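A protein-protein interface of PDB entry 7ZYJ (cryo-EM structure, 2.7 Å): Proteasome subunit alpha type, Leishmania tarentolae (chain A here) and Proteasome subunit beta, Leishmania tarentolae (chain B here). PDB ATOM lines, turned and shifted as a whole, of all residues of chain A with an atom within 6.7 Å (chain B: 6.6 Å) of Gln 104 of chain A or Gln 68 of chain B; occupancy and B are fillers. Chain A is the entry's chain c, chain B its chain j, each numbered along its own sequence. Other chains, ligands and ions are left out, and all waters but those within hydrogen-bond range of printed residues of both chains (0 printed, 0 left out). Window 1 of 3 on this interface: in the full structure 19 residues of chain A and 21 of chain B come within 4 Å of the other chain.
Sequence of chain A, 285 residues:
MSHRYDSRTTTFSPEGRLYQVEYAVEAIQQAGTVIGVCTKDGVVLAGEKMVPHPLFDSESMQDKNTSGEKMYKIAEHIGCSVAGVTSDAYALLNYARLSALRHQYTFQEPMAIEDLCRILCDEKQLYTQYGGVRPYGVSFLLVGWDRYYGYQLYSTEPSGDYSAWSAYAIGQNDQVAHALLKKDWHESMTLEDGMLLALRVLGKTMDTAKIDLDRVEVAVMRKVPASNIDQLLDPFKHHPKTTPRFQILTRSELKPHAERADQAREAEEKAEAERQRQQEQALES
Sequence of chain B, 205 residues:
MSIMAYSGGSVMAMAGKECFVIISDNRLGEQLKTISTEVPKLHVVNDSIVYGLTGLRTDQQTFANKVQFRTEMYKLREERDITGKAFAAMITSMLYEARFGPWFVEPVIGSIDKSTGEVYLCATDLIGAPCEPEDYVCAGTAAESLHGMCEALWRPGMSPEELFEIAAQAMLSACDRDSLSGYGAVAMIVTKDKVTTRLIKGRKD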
ATOM      1  N   HIS A  77      -0.886  19.519  -4.781  1.00  0.00           N
ATOM      2  CA  HIS A  77       0.027  18.405  -4.989  1.00  0.00           C
ATOM      3  C   HIS A  77       0.925  18.593  -6.205  1.00  0.00           C
ATOM      4  O   HIS A  77       1.640  17.660  -6.579  1.00  0.00           O
ATOM      5  CB  HIS A  77      -0.763  17.102  -5.125  1.00  0.00           C
ATOM      6  CG  HIS A  77      -1.570  17.012  -6.382  1.00  0.00           C
ATOM      7  ND1 HIS A  77      -2.679  17.795  -6.612  1.00  0.00           N
ATOM      8  CD2 HIS A  77      -1.434  16.222  -7.473  1.00  0.00           C
ATOM      9  CE1 HIS A  77      -3.188  17.498  -7.794  1.00  0.00           C
ATOM     10  NE2 HIS A  77      -2.452  16.546  -8.337  1.00  0.00           N
ATOM     11  N   SER A  99      -6.883  23.628 -15.477  1.00  0.00           N
ATOM     12  CA  SER A  99      -7.087  22.225 -15.831  1.00  0.00           C
ATOM     13  C   SER A  99      -7.096  21.332 -14.596  1.00  0.00           C
ATOM     14  O   SER A  99      -7.940  20.434 -14.477  1.00  0.00           O
ATOM     15  CB  SER A  99      -6.007  21.771 -16.812  1.00  0.00           C
ATOM     16  OG  SER A  99      -6.094  22.483 -18.032  1.00  0.00           O
ATOM     17  N   ALA A 100      -6.166  21.563 -13.665  1.00  0.00           N
ATOM     18  CA  ALA A 100      -6.133  20.762 -12.446  1.00  0.00           C
ATOM     19  C   ALA A 100      -7.398  20.949 -11.622  1.00  0.00           C
ATOM     20  O   ALA A 100      -7.968  19.970 -11.120  1.00  0.00           O
ATOM     21  CB  ALA A 100      -4.898  21.115 -11.618  1.00  0.00           C
ATOM     22  N   LEU A 101      -7.869  22.190 -11.488  1.00  0.00           N
ATOM     23  CA  LEU A 101      -9.086  22.420 -10.721  1.00  0.00           C
ATOM     24  C   LEU A 101     -10.323  21.891 -11.437  1.00  0.00           C
ATOM     25  O   LEU A 101     -11.269  21.458 -10.776  1.00  0.00           O
ATOM     26  CB  LEU A 101      -9.237  23.906 -10.409  1.00  0.00           C
ATOM     27  CG  LEU A 101      -8.238  24.413  -9.370  1.00  0.00           C
ATOM     28  CD1 LEU A 101      -8.439  25.889  -9.103  1.00  0.00           C
ATOM     29  CD2 LEU A 101      -8.350  23.607  -8.088  1.00  0.00           C
ATOM     30  N   ARG A 102     -10.335  21.898 -12.770  1.00  0.00           N
ATOM     31  CA  ARG A 102     -11.442  21.285 -13.498  1.00  0.00           C
ATOM     32  C   ARG A 102     -11.471  19.778 -13.283  1.00  0.00           C
ATOM     33  O   ARG A 102     -12.546  19.191 -13.101  1.00  0.00           O
ATOM     34  CB  ARG A 102     -11.336  21.613 -14.987  1.00  0.00           C
ATOM     35  CG  ARG A 102     -11.781  23.017 -15.342  1.00  0.00           C
ATOM     36  CD  ARG A 102     -12.093  23.138 -16.820  1.00  0.00           C
ATOM     37  NE  ARG A 102     -10.878  23.206 -17.623  1.00  0.00           N
ATOM     38  CZ  ARG A 102     -10.285  24.334 -17.988  1.00  0.00           C
ATOM     39  NH1 ARG A 102     -10.770  25.514 -17.638  1.00  0.00           N
ATOM     40  NH2 ARG A 102      -9.177  24.276 -18.720  1.00  0.00           N
ATOM     41  N   HIS A 103     -10.301  19.136 -13.302  1.00  0.00           N
ATOM     42  CA  HIS A 103     -10.250  17.707 -13.014  1.00  0.00           C
ATOM     43  C   HIS A 103     -10.725  17.417 -11.596  1.00  0.00           C
ATOM     44  O   HIS A 103     -11.453  16.445 -11.365  1.00  0.00           O
ATOM     45  CB  HIS A 103      -8.836  17.170 -13.223  1.00  0.00           C
ATOM     46  CG  HIS A 103      -8.699  15.710 -12.918  1.00  0.00           C
ATOM     47  ND1 HIS A 103      -8.830  14.734 -13.882  1.00  0.00           N
ATOM     48  CD2 HIS A 103      -8.450  15.060 -11.757  1.00  0.00           C
ATOM     49  CE1 HIS A 103      -8.664  13.547 -13.328  1.00  0.00           C
ATOM     50  NE2 HIS A 103      -8.433  13.717 -12.040  1.00  0.00           N
ATOM     51  N   GLN A 104     -10.317  18.246 -10.633  1.00  0.00           N
ATOM     52  CA  GLN A 104     -10.804  18.072  -9.267  1.00  0.00           C
ATOM     53  C   GLN A 104     -12.310  18.290  -9.180  1.00  0.00           C
ATOM     54  O   GLN A 104     -12.990  17.617  -8.398  1.00  0.00           O
ATOM     55  CB  GLN A 104     -10.068  19.018  -8.320  1.00  0.00           C
ATOM     56  CG  GLN A 104     -10.685  19.116  -6.935  1.00  0.00           C
ATOM     57  CD  GLN A 104      -9.644  19.224  -5.842  1.00  0.00           C
ATOM     58  OE1 GLN A 104      -8.628  18.529  -5.864  1.00  0.00           O
ATOM     59  NE2 GLN A 104      -9.891  20.098  -4.873  1.00  0.00           N
ATOM     60  N   TYR A 105     -12.848  19.220  -9.967  1.00  0.00           N
ATOM     61  CA  TYR A 105     -14.289  19.430 -10.003  1.00  0.00           C
ATOM     62  C   TYR A 105     -15.016  18.202 -10.534  1.00  0.00           C
ATOM     63  O   TYR A 105     -16.053  17.805  -9.991  1.00  0.00           O
ATOM     64  CB  TYR A 105     -14.611  20.655 -10.860  1.00  0.00           C
ATOM     65  CG  TYR A 105     -16.085  20.950 -11.008  1.00  0.00           C
ATOM     66  CD1 TYR A 105     -16.752  21.740 -10.083  1.00  0.00           C
ATOM     67  CD2 TYR A 105     -16.810  20.446 -12.081  1.00  0.00           C
ATOM     68  CE1 TYR A 105     -18.099  22.015 -10.218  1.00  0.00           C
ATOM     69  CE2 TYR A 105     -18.155  20.714 -12.223  1.00  0.00           C
ATOM     70  CZ  TYR A 105     -18.794  21.498 -11.289  1.00  0.00           C
ATOM     71  OH  TYR A 105     -20.135  21.770 -11.426  1.00  0.00           O
ATOM     72  N   THR A 106     -14.490  17.591 -11.595  1.00  0.00           N
ATOM     73  CA  THR A 106     -15.196  16.485 -12.231  1.00  0.00           C
ATOM     74  C   THR A 106     -15.117  15.201 -11.410  1.00  0.00           C
ATOM     75  O   THR A 106     -16.116  14.485 -11.278  1.00  0.00           O
ATOM     76  CB  THR A 106     -14.643  16.249 -13.637  1.00  0.00           C
ATOM     77  OG1 THR A 106     -14.821  17.434 -14.422  1.00  0.00           O
ATOM     78  CG2 THR A 106     -15.367  15.096 -14.308  1.00  0.00           C
ATOM     79  N   PHE A 107     -13.950  14.894 -10.843  1.00  0.00           N
ATOM     80  CA  PHE A 107     -13.723  13.603 -10.211  1.00  0.00           C
ATOM     81  C   PHE A 107     -13.533  13.671  -8.704  1.00  0.00           C
ATOM     82  O   PHE A 107     -13.548  12.620  -8.054  1.00  0.00           O
ATOM     83  CB  PHE A 107     -12.499  12.918 -10.839  1.00  0.00           C
ATOM     84  CG  PHE A 107     -12.661  12.614 -12.300  1.00  0.00           C
ATOM     85  CD1 PHE A 107     -13.284  11.449 -12.716  1.00  0.00           C
ATOM     86  CD2 PHE A 107     -12.191  13.492 -13.259  1.00  0.00           C
ATOM     87  CE1 PHE A 107     -13.433  11.170 -14.057  1.00  0.00           C
ATOM     88  CE2 PHE A 107     -12.337  13.217 -14.604  1.00  0.00           C
ATOM     89  CZ  PHE A 107     -12.959  12.054 -15.002  1.00  0.00           C
ATOM     90  N   GLN A 108     -13.356  14.864  -8.133  1.00  0.00           N
ATOM     91  CA  GLN A 108     -13.114  15.037  -6.699  1.00  0.00           C
ATOM     92  C   GLN A 108     -11.882  14.267  -6.231  1.00  0.00           C
ATOM     93  O   GLN A 108     -11.846  13.751  -5.113  1.00  0.00           O
ATOM     94  CB  GLN A 108     -14.340  14.642  -5.871  1.00  0.00           C
ATOM     95  CG  GLN A 108     -15.615  15.368  -6.267  1.00  0.00           C
ATOM     96  CD  GLN A 108     -15.516  16.866  -6.071  1.00  0.00           C
ATOM     97  OE1 GLN A 108     -15.186  17.341  -4.985  1.00  0.00           O
ATOM     98  NE2 GLN A 108     -15.802  17.620  -7.124  1.00  0.00           N
ATOM     99  N   GLU A 109     -10.867  14.187  -7.084  1.00  0.00           N
ATOM    100  CA  GLU A 109      -9.590  13.580  -6.747  1.00  0.00           C
ATOM    101  C   GLU A 109      -8.477  14.436  -7.330  1.00  0.00           C
ATOM    102  O   GLU A 109      -8.688  15.136  -8.328  1.00  0.00           O
ATOM    103  CB  GLU A 109      -9.471  12.147  -7.288  1.00  0.00           C
ATOM    104  CG  GLU A 109      -9.458  12.056  -8.802  1.00  0.00           C
ATOM    105  CD  GLU A 109      -9.402  10.628  -9.300  1.00  0.00           C
ATOM    106  OE1 GLU A 109      -9.397   9.704  -8.459  1.00  0.00           O
ATOM    107  OE2 GLU A 109      -9.363  10.428 -10.531  1.00  0.00           O
ATOM    108  N   PRO A 110      -7.291  14.415  -6.722  1.00  0.00           N
ATOM    109  CA  PRO A 110      -6.161  15.152  -7.301  1.00  0.00           C
ATOM    110  C   PRO A 110      -5.802  14.625  -8.681  1.00  0.00           C
ATOM    111  O   PRO A 110      -5.811  13.418  -8.928  1.00  0.00           O
ATOM    112  CB  PRO A 110      -5.028  14.913  -6.297  1.00  0.00           C
ATOM    113  CG  PRO A 110      -5.712  14.545  -5.025  1.00  0.00           C
ATOM    114  CD  PRO A 110      -6.950  13.807  -5.426  1.00  0.00           C
ATOM    115  N   MET A 111      -5.484  15.550  -9.582  1.00  0.00           N
ATOM    116  CA  MET A 111      -5.073  15.179 -10.927  1.00  0.00           C
ATOM    117  C   MET A 111      -3.710  14.501 -10.902  1.00  0.00           C
ATOM    118  O   MET A 111      -2.811  14.904 -10.158  1.00  0.00           O
ATOM    119  CB  MET A 111      -5.026  16.411 -11.828  1.00  0.00           C
ATOM    120  CG  MET A 111      -5.317  16.129 -13.290  1.00  0.00           C
ATOM    121  SD  MET A 111      -5.130  17.596 -14.319  1.00  0.00           S
ATOM    122  CE  MET A 111      -5.740  16.990 -15.889  1.00  0.00           C
ATOM    123  N   TYR B  51     -19.420  27.365   5.989  1.00  0.00           N
ATOM    124  CA  TYR B  51     -20.725  27.616   5.403  1.00  0.00           C
ATOM    125  C   TYR B  51     -21.466  26.304   5.184  1.00  0.00           C
ATOM    126  O   TYR B  51     -20.866  25.244   4.996  1.00  0.00           O
ATOM    127  CB  TYR B  51     -20.613  28.390   4.082  1.00  0.00           C
ATOM    128  CG  TYR B  51     -20.305  27.538   2.874  1.00  0.00           C
ATOM    129  CD1 TYR B  51     -19.032  27.032   2.663  1.00  0.00           C
ATOM    130  CD2 TYR B  51     -21.289  27.248   1.940  1.00  0.00           C
ATOM    131  CE1 TYR B  51     -18.747  26.259   1.557  1.00  0.00           C
ATOM    132  CE2 TYR B  51     -21.015  26.473   0.834  1.00  0.00           C
ATOM    133  CZ  TYR B  51     -19.742  25.981   0.648  1.00  0.00           C
ATOM    134  OH  TYR B  51     -19.465  25.208  -0.455  1.00  0.00           O
ATOM    135  N   PHE B  63     -23.279  23.084  -6.211  1.00  0.00           N
ATOM    136  CA  PHE B  63     -22.857  24.403  -5.764  1.00  0.00           C
ATOM    137  C   PHE B  63     -21.642  24.323  -4.851  1.00  0.00           C
ATOM    138  O   PHE B  63     -20.773  25.196  -4.911  1.00  0.00           O
ATOM    139  CB  PHE B  63     -24.012  25.113  -5.058  1.00  0.00           C
ATOM    140  CG  PHE B  63     -23.794  26.585  -4.876  1.00  0.00           C
ATOM    141  CD1 PHE B  63     -23.949  27.457  -5.940  1.00  0.00           C
ATOM    142  CD2 PHE B  63     -23.429  27.098  -3.643  1.00  0.00           C
ATOM    143  CE1 PHE B  63     -23.745  28.813  -5.777  1.00  0.00           C
ATOM    144  CE2 PHE B  63     -23.225  28.452  -3.475  1.00  0.00           C
ATOM    145  CZ  PHE B  63     -23.383  29.310  -4.542  1.00  0.00           C
ATOM    146  N   ALA B  64     -21.561  23.294  -4.003  1.00  0.00           N
ATOM    147  CA  ALA B  64     -20.380  23.127  -3.164  1.00  0.00           C
ATOM    148  C   ALA B  64     -19.142  22.856  -4.004  1.00  0.00           C
ATOM    149  O   ALA B  64     -18.061  23.378  -3.712  1.00  0.00           O
ATOM    150  CB  ALA B  64     -20.606  22.002  -2.155  1.00  0.00           C
ATOM    151  N   ASN B  65     -19.276  22.041  -5.055  1.00  0.00           N
ATOM    152  CA  ASN B  65     -18.147  21.804  -5.948  1.00  0.00           C
ATOM    153  C   ASN B  65     -17.722  23.088  -6.651  1.00  0.00           C
ATOM    154  O   ASN B  65     -16.524  23.372  -6.774  1.00  0.00           O
ATOM    155  CB  ASN B  65     -18.502  20.725  -6.970  1.00  0.00           C
ATOM    156  CG  ASN B  65     -18.711  19.368  -6.335  1.00  0.00           C
ATOM    157  OD1 ASN B  65     -18.431  19.173  -5.152  1.00  0.00           O
ATOM    158  ND2 ASN B  65     -19.208  18.419  -7.118  1.00  0.00           N
ATOM    159  N   LYS B  66     -18.693  23.877  -7.118  1.00  0.00           N
ATOM    160  CA  LYS B  66     -18.366  25.147  -7.760  1.00  0.00           C
ATOM    161  C   LYS B  66     -17.667  26.093  -6.791  1.00  0.00           C
ATOM    162  O   LYS B  66     -16.699  26.770  -7.160  1.00  0.00           O
ATOM    163  CB  LYS B  66     -19.633  25.792  -8.320  1.00  0.00           C
ATOM    164  CG  LYS B  66     -20.118  25.172  -9.615  1.00  0.00           C
ATOM    165  CD  LYS B  66     -21.427  25.794 -10.063  1.00  0.00           C
ATOM    166  CE  LYS B  66     -21.595  25.693 -11.568  1.00  0.00           C
ATOM    167  NZ  LYS B  66     -21.928  24.307 -11.995  1.00  0.00           N
ATOM    168  N   VAL B  67     -18.143  26.154  -5.548  1.00  0.00           N
ATOM    169  CA  VAL B  67     -17.534  27.025  -4.549  1.00  0.00           C
ATOM    170  C   VAL B  67     -16.120  26.562  -4.225  1.00  0.00           C
ATOM    171  O   VAL B  67     -15.214  27.380  -4.046  1.00  0.00           O
ATOM    172  CB  VAL B  67     -18.418  27.088  -3.291  1.00  0.00           C
ATOM    173  CG1 VAL B  67     -17.657  27.695  -2.129  1.00  0.00           C
ATOM    174  CG2 VAL B  67     -19.675  27.891  -3.572  1.00  0.00           C
ATOM    175  N   GLN B  68     -15.909  25.249  -4.132  1.00  0.00           N
ATOM    176  CA  GLN B  68     -14.567  24.730  -3.891  1.00  0.00           C
ATOM    177  C   GLN B  68     -13.631  25.101  -5.033  1.00  0.00           C
ATOM    178  O   GLN B  68     -12.497  25.539  -4.803  1.00  0.00           O
ATOM    179  CB  GLN B  68     -14.618  23.214  -3.705  1.00  0.00           C
ATOM    180  CG  GLN B  68     -13.422  22.635  -2.973  1.00  0.00           C
ATOM    181  CD  GLN B  68     -13.113  21.215  -3.403  1.00  0.00           C
ATOM    182  OE1 GLN B  68     -13.763  20.669  -4.294  1.00  0.00           O
ATOM    183  NE2 GLN B  68     -12.117  20.609  -2.768  1.00  0.00           N
ATOM    184  N   PHE B  69     -14.097  24.939  -6.274  1.00  0.00           N
ATOM    185  CA  PHE B  69     -13.315  25.358  -7.434  1.00  0.00           C
ATOM    186  C   PHE B  69     -12.942  26.833  -7.333  1.00  0.00           C
ATOM    187  O   PHE B  69     -11.778  27.212  -7.519  1.00  0.00           O
ATOM    188  CB  PHE B  69     -14.116  25.079  -8.710  1.00  0.00           C
ATOM    189  CG  PHE B  69     -13.449  25.544  -9.978  1.00  0.00           C
ATOM    190  CD1 PHE B  69     -13.589  26.852 -10.417  1.00  0.00           C
ATOM    191  CD2 PHE B  69     -12.703  24.667 -10.743  1.00  0.00           C
ATOM    192  CE1 PHE B  69     -12.981  27.277 -11.581  1.00  0.00           C
ATOM    193  CE2 PHE B  69     -12.097  25.086 -11.911  1.00  0.00           C
ATOM    194  CZ  PHE B  69     -12.234  26.391 -12.329  1.00  0.00           C
ATOM    195  N   ARG B  70     -13.929  27.676  -7.023  1.00  0.00           N
ATOM    196  CA  ARG B  70     -13.696  29.115  -6.984  1.00  0.00           C
ATOM    197  C   ARG B  70     -12.725  29.497  -5.873  1.00  0.00           C
ATOM    198  O   ARG B  70     -11.838  30.330  -6.082  1.00  0.00           O
ATOM    199  CB  ARG B  70     -15.023  29.852  -6.818  1.00  0.00           C
ATOM    200  CG  ARG B  70     -15.825  29.956  -8.101  1.00  0.00           C
ATOM    201  CD  ARG B  70     -15.144  30.881  -9.093  1.00  0.00           C
ATOM    202  NE  ARG B  70     -15.553  32.269  -8.921  1.00  0.00           N
ATOM    203  CZ  ARG B  70     -16.735  32.754  -9.276  1.00  0.00           C
ATOM    204  NH1 ARG B  70     -17.649  31.993  -9.857  1.00  0.00           N
ATOM    205  NH2 ARG B  70     -17.004  34.036  -9.050  1.00  0.00           N
ATOM    206  N   THR B  71     -12.867  28.896  -4.690  1.00  0.00           N
ATOM    207  CA  THR B  71     -11.983  29.238  -3.580  1.00  0.00           C
ATOM    208  C   THR B  71     -10.563  28.744  -3.821  1.00  0.00           C
ATOM    209  O   THR B  71      -9.597  29.434  -3.475  1.00  0.00           O
ATOM    210  CB  THR B  71     -12.526  28.678  -2.265  1.00  0.00           C
ATOM    211  OG1 THR B  71     -12.637  27.252  -2.354  1.00  0.00           O
ATOM    212  CG2 THR B  71     -13.880  29.285  -1.937  1.00  0.00           C
ATOM    213  N   GLU B  72     -10.405  27.555  -4.410  1.00  0.00           N
ATOM    214  CA  GLU B  72      -9.062  27.089  -4.737  1.00  0.00           C
ATOM    215  C   GLU B  72      -8.410  27.979  -5.787  1.00  0.00           C
ATOM    216  O   GLU B  72      -7.222  28.307  -5.675  1.00  0.00           O
ATOM    217  CB  GLU B  72      -9.098  25.635  -5.207  1.00  0.00           C
ATOM    218  CG  GLU B  72      -9.607  24.652  -4.166  1.00  0.00           C
ATOM    219  CD  GLU B  72      -8.885  24.774  -2.839  1.00  0.00           C
ATOM    220  OE1 GLU B  72      -7.647  24.933  -2.841  1.00  0.00           O
ATOM    221  OE2 GLU B  72      -9.561  24.713  -1.790  1.00  0.00           O
ATOM    222  N   MET B  73      -9.166  28.387  -6.809  1.00  0.00           N
ATOM    223  CA  MET B  73      -8.616  29.300  -7.804  1.00  0.00           C
ATOM    224  C   MET B  73      -8.252  30.641  -7.180  1.00  0.00           C
ATOM    225  O   MET B  73      -7.225  31.237  -7.522  1.00  0.00           O
ATOM    226  CB  MET B  73      -9.608  29.491  -8.950  1.00  0.00           C
ATOM    227  CG  MET B  73      -8.982  30.012 -10.232  1.00  0.00           C
ATOM    228  SD  MET B  73      -7.761  28.885 -10.930  1.00  0.00           S
ATOM    229  CE  MET B  73      -6.243  29.775 -10.606  1.00  0.00           C
ATOM    230  N   MET B  90     -18.908  36.723  -3.347  1.00  0.00           N
ATOM    231  CA  MET B  90     -18.701  35.798  -4.454  1.00  0.00           C
ATOM    232  C   MET B  90     -19.870  34.828  -4.581  1.00  0.00           C
ATOM    233  O   MET B  90     -20.332  34.540  -5.690  1.00  0.00           O
ATOM    234  CB  MET B  90     -17.381  35.048  -4.268  1.00  0.00           C
ATOM    235  CG  MET B  90     -17.198  33.851  -5.185  1.00  0.00           C
ATOM    236  SD  MET B  90     -15.812  32.812  -4.689  1.00  0.00           S
ATOM    237  CE  MET B  90     -16.667  31.472  -3.869  1.00  0.00           C
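Of chain A, only Gln 104 (3.1 Å) and Gln 108 (3.7 Å) come within 4 Å of Gln 68 of chain B.
Printed residues of chain B within 4 Å of Tyr 105 of chain A: Asn 65 (3.5 Å) and Lys 66 (3.2 Å).
Of the printed residues of chain A, Met 73 of chain B touches Leu 101.
Thr 71 of chain B touches none of the printed residues of chain A.
The side-chain amide nitrogen (ND2) of Asn 65 of chain B lies close to the side-chain amide nitrogen (NE2) of Gln 108 of chain A (3.5 Å).
OH of Tyr 105 of chain A lies within hydrogen-bond range of NZ of Lys 66 of chain B, 3.2 Å away.
NE2 of Gln 68 of chain B sits close to NE2 of Gln 104 of chain A, 3.1 Å away.
CB of Leu 101 of chain A touches CE2 of Phe 69 of chain B, 3.4 Å away.
Leu 101 of chain A touches Glu 72 of chain B.
N of Met 73 of chain B touches CD1 of Leu 101 of chain A, 3.5 Å away.
CE2 of Phe 69 of chain B touches N of Arg 102 of chain A (3.7 Å).
CE1 of Tyr 105 of chain A touches CB of Asn 65 of chain B, 3.5 Å away.
Gln 108 of chain A touches Gln 68 of chain B (OE1 to OE1, 3.7 Å).
The backbone carbonyl oxygen (O) of Gln 68 of chain B lies within hydrogen-bond range of the side-chain hydroxyl (OG1) of Thr 71 of chain B (3.0 Å).
OG1 of Thr 106 of chain A is in hydrogen-bond range of O of Arg 102 of chain A, 3.2 Å away.
O of Gln 104 of chain A is in hydrogen-bond range of NE2 of Gln 108 of chain A.
NE2 of Gln 108 of chain A sits at hydrogen-bond distance from O of Tyr 105 of chain A (2.9 Å).
Printed residues of chain B that touch a printed residue of chain A: Asn 65, Lys 66, Gln 68, Phe 69, Glu 72 and Met 73.
Hydrophobic or aromatic side chains of chain A within 4 Å of the printed part of chain B: Leu 101 and Tyr 105.
Among the printed residues, 9 pairs touch across the chains.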
